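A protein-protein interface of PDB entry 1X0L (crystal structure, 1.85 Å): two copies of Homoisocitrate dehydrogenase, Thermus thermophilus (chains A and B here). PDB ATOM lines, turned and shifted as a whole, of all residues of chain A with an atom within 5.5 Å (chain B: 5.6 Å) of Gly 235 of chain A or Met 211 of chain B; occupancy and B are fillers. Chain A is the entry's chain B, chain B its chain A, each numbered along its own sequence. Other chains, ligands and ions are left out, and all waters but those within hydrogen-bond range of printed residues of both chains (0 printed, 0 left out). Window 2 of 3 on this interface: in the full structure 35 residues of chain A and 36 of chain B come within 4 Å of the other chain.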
ATOM      1  N   GLY A 106      -8.576 -10.057  12.759  1.00  0.00           N
ATOM      2  CA  GLY A 106      -9.385 -11.249  12.933  1.00  0.00           C
ATOM      3  C   GLY A 106      -8.543 -12.405  13.436  1.00  0.00           C
ATOM      4  O   GLY A 106      -8.898 -13.571  13.258  1.00  0.00           O
ATOM      5  N   SER A 230      -7.378 -28.810  14.708  1.00  0.00           N
ATOM      6  CA  SER A 230      -6.614 -27.959  13.804  1.00  0.00           C
ATOM      7  C   SER A 230      -7.490 -26.927  13.098  1.00  0.00           C
ATOM      8  O   SER A 230      -7.068 -25.789  12.888  1.00  0.00           O
ATOM      9  CB  SER A 230      -5.878 -28.811  12.764  1.00  0.00           C
ATOM     10  OG  SER A 230      -4.785 -29.478  13.364  1.00  0.00           O
ATOM     11  N   ASP A 231      -8.701 -27.323  12.723  1.00  0.00           N
ATOM     12  CA  ASP A 231      -9.606 -26.395  12.057  1.00  0.00           C
ATOM     13  C   ASP A 231     -10.120 -25.380  13.065  1.00  0.00           C
ATOM     14  O   ASP A 231     -10.354 -24.219  12.726  1.00  0.00           O
ATOM     15  CB  ASP A 231     -10.769 -27.137  11.404  1.00  0.00           C
ATOM     16  CG  ASP A 231     -10.411 -27.673  10.030  1.00  0.00           C
ATOM     17  OD1 ASP A 231     -11.325 -28.127   9.314  1.00  0.00           O
ATOM     18  OD2 ASP A 231      -9.218 -27.636   9.666  1.00  0.00           O
ATOM     19  N   LEU A 232     -10.292 -25.825  14.304  1.00  0.00           N
ATOM     20  CA  LEU A 232     -10.738 -24.941  15.369  1.00  0.00           C
ATOM     21  C   LEU A 232      -9.644 -23.889  15.520  1.00  0.00           C
ATOM     22  O   LEU A 232      -9.909 -22.685  15.501  1.00  0.00           O
ATOM     23  CB  LEU A 232     -10.896 -25.731  16.673  1.00  0.00           C
ATOM     24  CG  LEU A 232     -11.391 -25.012  17.931  1.00  0.00           C
ATOM     25  CD1 LEU A 232     -11.698 -26.041  18.998  1.00  0.00           C
ATOM     26  CD2 LEU A 232     -10.355 -24.017  18.432  1.00  0.00           C
ATOM     27  N   ALA A 233      -8.407 -24.360  15.661  1.00  0.00           N
ATOM     28  CA  ALA A 233      -7.254 -23.481  15.821  1.00  0.00           C
ATOM     29  C   ALA A 233      -7.109 -22.507  14.658  1.00  0.00           C
ATOM     30  O   ALA A 233      -6.781 -21.337  14.855  1.00  0.00           O
ATOM     31  CB  ALA A 233      -5.982 -24.310  15.963  1.00  0.00           C
ATOM     32  N   ALA A 234      -7.340 -22.989  13.442  1.00  0.00           N
ATOM     33  CA  ALA A 234      -7.231 -22.124  12.275  1.00  0.00           C
ATOM     34  C   ALA A 234      -8.241 -20.994  12.414  1.00  0.00           C
ATOM     35  O   ALA A 234      -7.964 -19.852  12.054  1.00  0.00           O
ATOM     36  CB  ALA A 234      -7.496 -22.916  10.997  1.00  0.00           C
ATOM     37  N   GLY A 235      -9.413 -21.322  12.950  1.00  0.00           N
ATOM     38  CA  GLY A 235     -10.449 -20.322  13.125  1.00  0.00           C
ATOM     39  C   GLY A 235     -10.010 -19.190  14.036  1.00  0.00           C
ATOM     40  O   GLY A 235     -10.490 -18.063  13.911  1.00  0.00           O
ATOM     41  N   LEU A 236      -9.083 -19.491  14.942  1.00  0.00           N
ATOM     42  CA  LEU A 236      -8.579 -18.510  15.899  1.00  0.00           C
ATOM     43  C   LEU A 236      -7.531 -17.557  15.339  1.00  0.00           C
ATOM     44  O   LEU A 236      -7.409 -16.425  15.811  1.00  0.00           O
ATOM     45  CB  LEU A 236      -7.970 -19.224  17.108  1.00  0.00           C
ATOM     46  CG  LEU A 236      -8.867 -20.120  17.959  1.00  0.00           C
ATOM     47  CD1 LEU A 236      -8.002 -20.972  18.868  1.00  0.00           C
ATOM     48  CD2 LEU A 236      -9.829 -19.267  18.766  1.00  0.00           C
ATOM     49  N   VAL A 237      -6.775 -18.005  14.342  1.00  0.00           N
ATOM     50  CA  VAL A 237      -5.715 -17.174  13.783  1.00  0.00           C
ATOM     51  C   VAL A 237      -5.882 -16.682  12.345  1.00  0.00           C
ATOM     52  O   VAL A 237      -4.901 -16.288  11.712  1.00  0.00           O
ATOM     53  CB  VAL A 237      -4.358 -17.895  13.887  1.00  0.00           C
ATOM     54  CG1 VAL A 237      -4.007 -18.128  15.346  1.00  0.00           C
ATOM     55  CG2 VAL A 237      -4.416 -19.219  13.138  1.00  0.00           C
ATOM     56  N   GLY A 238      -7.103 -16.703  11.822  1.00  0.00           N
ATOM     57  CA  GLY A 238      -7.306 -16.215  10.467  1.00  0.00           C
ATOM     58  C   GLY A 238      -7.905 -17.169   9.448  1.00  0.00           C
ATOM     59  O   GLY A 238      -7.986 -16.834   8.263  1.00  0.00           O
ATOM     60  N   GLY A 239      -8.329 -18.348   9.889  1.00  0.00           N
ATOM     61  CA  GLY A 239      -8.916 -19.306   8.969  1.00  0.00           C
ATOM     62  C   GLY A 239      -7.875 -20.152   8.260  1.00  0.00           C
ATOM     63  O   GLY A 239      -6.676 -19.927   8.413  1.00  0.00           O
ATOM     64  N   ARG B 108     -18.704 -14.328  25.103  1.00  0.00           N
ATOM     65  CA  ARG B 108     -18.823 -13.588  23.855  1.00  0.00           C
ATOM     66  C   ARG B 108     -20.311 -13.377  23.578  1.00  0.00           C
ATOM     67  O   ARG B 108     -21.117 -14.272  23.808  1.00  0.00           O
ATOM     68  CB  ARG B 108     -18.194 -14.406  22.723  1.00  0.00           C
ATOM     69  CG  ARG B 108     -18.318 -13.804  21.341  1.00  0.00           C
ATOM     70  CD  ARG B 108     -17.746 -14.759  20.298  1.00  0.00           C
ATOM     71  NE  ARG B 108     -17.812 -14.218  18.943  1.00  0.00           N
ATOM     72  CZ  ARG B 108     -18.933 -13.833  18.340  1.00  0.00           C
ATOM     73  NH1 ARG B 108     -18.892 -13.356  17.104  1.00  0.00           N
ATOM     74  NH2 ARG B 108     -20.096 -13.922  18.971  1.00  0.00           N
ATOM     75  N   ALA B 206     -16.720 -26.493  13.018  1.00  0.00           N
ATOM     76  CA  ALA B 206     -15.861 -26.095  14.125  1.00  0.00           C
ATOM     77  C   ALA B 206     -15.243 -24.732  13.851  1.00  0.00           C
ATOM     78  O   ALA B 206     -15.261 -23.848  14.706  1.00  0.00           O
ATOM     79  CB  ALA B 206     -14.764 -27.131  14.338  1.00  0.00           C
ATOM     80  N   MET B 207     -14.693 -24.559  12.653  1.00  0.00           N
ATOM     81  CA  MET B 207     -14.067 -23.291  12.302  1.00  0.00           C
ATOM     82  C   MET B 207     -15.076 -22.151  12.310  1.00  0.00           C
ATOM     83  O   MET B 207     -14.820 -21.087  12.874  1.00  0.00           O
ATOM     84  CB  MET B 207     -13.412 -23.381  10.924  1.00  0.00           C
ATOM     85  CG  MET B 207     -12.556 -22.174  10.586  1.00  0.00           C
ATOM     86  SD  MET B 207     -11.812 -22.315   8.955  1.00  0.00           S
ATOM     87  CE  MET B 207     -11.290 -24.023   8.997  1.00  0.00           C
ATOM     88  N   GLN B 208     -16.231 -22.369  11.687  1.00  0.00           N
ATOM     89  CA  GLN B 208     -17.247 -21.328  11.648  1.00  0.00           C
ATOM     90  C   GLN B 208     -17.784 -20.970  13.034  1.00  0.00           C
ATOM     91  O   GLN B 208     -18.110 -19.813  13.292  1.00  0.00           O
ATOM     92  CB  GLN B 208     -18.390 -21.733  10.715  1.00  0.00           C
ATOM     93  CG  GLN B 208     -17.954 -21.854   9.257  1.00  0.00           C
ATOM     94  CD  GLN B 208     -19.120 -21.985   8.297  1.00  0.00           C
ATOM     95  OE1 GLN B 208     -18.938 -22.332   7.128  1.00  0.00           O
ATOM     96  NE2 GLN B 208     -20.324 -21.699   8.780  1.00  0.00           N
ATOM     97  N   LEU B 209     -17.869 -21.949  13.931  1.00  0.00           N
ATOM     98  CA  LEU B 209     -18.359 -21.667  15.282  1.00  0.00           C
ATOM     99  C   LEU B 209     -17.437 -20.672  15.980  1.00  0.00           C
ATOM    100  O   LEU B 209     -17.884 -19.837  16.769  1.00  0.00           O
ATOM    101  CB  LEU B 209     -18.436 -22.952  16.111  1.00  0.00           C
ATOM    102  CG  LEU B 209     -19.659 -23.840  15.878  1.00  0.00           C
ATOM    103  CD1 LEU B 209     -19.433 -25.202  16.521  1.00  0.00           C
ATOM    104  CD2 LEU B 209     -20.900 -23.154  16.460  1.00  0.00           C
ATOM    105  N   VAL B 210     -16.145 -20.767  15.694  1.00  0.00           N
ATOM    106  CA  VAL B 210     -15.177 -19.869  16.306  1.00  0.00           C
ATOM    107  C   VAL B 210     -15.209 -18.491  15.655  1.00  0.00           C
ATOM    108  O   VAL B 210     -15.068 -17.473  16.336  1.00  0.00           O
ATOM    109  CB  VAL B 210     -13.740 -20.443  16.206  1.00  0.00           C
ATOM    110  CG1 VAL B 210     -12.727 -19.426  16.714  1.00  0.00           C
ATOM    111  CG2 VAL B 210     -13.638 -21.722  17.021  1.00  0.00           C
ATOM    112  N   MET B 211     -15.419 -18.458  14.341  1.00  0.00           N
ATOM    113  CA  MET B 211     -15.432 -17.197  13.602  1.00  0.00           C
ATOM    114  C   MET B 211     -16.783 -16.493  13.485  1.00  0.00           C
ATOM    115  O   MET B 211     -16.854 -15.268  13.588  1.00  0.00           O
ATOM    116  CB  MET B 211     -14.851 -17.417  12.201  1.00  0.00           C
ATOM    117  CG  MET B 211     -13.443 -18.007  12.203  1.00  0.00           C
ATOM    118  SD  MET B 211     -12.747 -18.231  10.547  1.00  0.00           S
ATOM    119  CE  MET B 211     -14.000 -19.210   9.781  1.00  0.00           C
ATOM    120  N   ARG B 212     -17.853 -17.251  13.270  1.00  0.00           N
ATOM    121  CA  ARG B 212     -19.174 -16.650  13.129  1.00  0.00           C
ATOM    122  C   ARG B 212     -20.246 -17.528  13.766  1.00  0.00           C
ATOM    123  O   ARG B 212     -21.109 -18.068  13.084  1.00  0.00           O
ATOM    124  CB  ARG B 212     -19.656 -16.765  11.681  1.00  0.00           C
ATOM    125  CG  ARG B 212     -18.910 -15.866  10.706  1.00  0.00           C
ATOM    126  CD  ARG B 212     -18.986 -16.407   9.288  1.00  0.00           C
ATOM    127  NE  ARG B 212     -20.266 -17.052   9.016  1.00  0.00           N
ATOM    128  CZ  ARG B 212     -20.586 -17.609   7.852  1.00  0.00           C
ATOM    129  NH1 ARG B 212     -19.719 -17.612   6.851  1.00  0.00           N
ATOM    130  NH2 ARG B 212     -21.778 -18.163   7.692  1.00  0.00           N
ATOM    131  N   PRO B 213     -20.216 -17.669  15.101  1.00  0.00           N
ATOM    132  CA  PRO B 213     -21.199 -18.499  15.805  1.00  0.00           C
ATOM    133  C   PRO B 213     -22.659 -18.085  15.606  1.00  0.00           C
ATOM    134  O   PRO B 213     -23.566 -18.909  15.744  1.00  0.00           O
ATOM    135  CB  PRO B 213     -20.747 -18.402  17.262  1.00  0.00           C
ATOM    136  CG  PRO B 213     -20.126 -17.029  17.332  1.00  0.00           C
ATOM    137  CD  PRO B 213     -19.334 -16.967  16.050  1.00  0.00           C
ATOM    138  N   GLU B 214     -22.893 -16.820  15.268  1.00  0.00           N
ATOM    139  CA  GLU B 214     -24.262 -16.344  15.069  1.00  0.00           C
ATOM    140  C   GLU B 214     -24.978 -16.971  13.880  1.00  0.00           C
ATOM    141  O   GLU B 214     -26.191 -16.826  13.728  1.00  0.00           O
ATOM    142  CB  GLU B 214     -24.290 -14.815  14.926  1.00  0.00           C
ATOM    143  CG  GLU B 214     -23.115 -14.232  14.171  1.00  0.00           C
ATOM    144  CD  GLU B 214     -21.870 -14.158  15.028  1.00  0.00           C
ATOM    145  OE1 GLU B 214     -21.914 -13.488  16.085  1.00  0.00           O
ATOM    146  OE2 GLU B 214     -20.852 -14.765  14.653  1.00  0.00           O
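Among the printed residues, pairs that only touch across the chains: Asp 231 of chain A with Met 207 of chain B (3.6 Å), Gly 235 of chain A with Met 207 of chain B (3.8 Å), Gly 235 of chain A with Val 210 of chain B (3.8 Å), Gly 235 of chain A with Met 211 of chain B (3.4 Å) and Leu 236 of chain A with Val 210 of chain B (3.6 Å).
Ala 234 of chain A touches none of the printed residues of chain B. Gly 235 of chain A touches three residues of chain B. Printed residues of chain B within 4 Å of Leu 236 of chain A: Val 210 (3.6 Å). Of the printed residues of chain A, Met 207 of chain B touches Asp 231 and Gly 235. Leu 209 of chain B touches none of the printed residues of chain A. Printed residues of chain A within 4 Å of Val 210 of chain B: Gly 235 (3.8 Å) and Leu 236 (3.6 Å). Met 211 of chain B touches just one residue of chain A: Gly 235. The nearest residue of chain A that does not touch Met 211 of chain B is Gly 239 of chain A (4.3 Å). The nearest printed residue of chain A that does not touch Val 210 of chain B is Leu 232 of chain A (4.1 Å).
Hydrophobic or aromatic side chains of chain A within 4 Å of the printed part of chain B: Leu 236. Of the 10 printed residues of chain B, 3 touch a printed residue of chain A. Printed residues of chain B that touch a printed residue of chain A: Met 207, Val 210 and Met 211. Hydrophobic or aromatic side chains of chain B that line the printed part of chain A: Met 207, Val 210 and Met 211. Along chain B the printed residues that touch a printed residue of chain A span positions 207 to 211. Among the printed residues, 5 pairs touch across the chains.
No position is printed for both chains.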
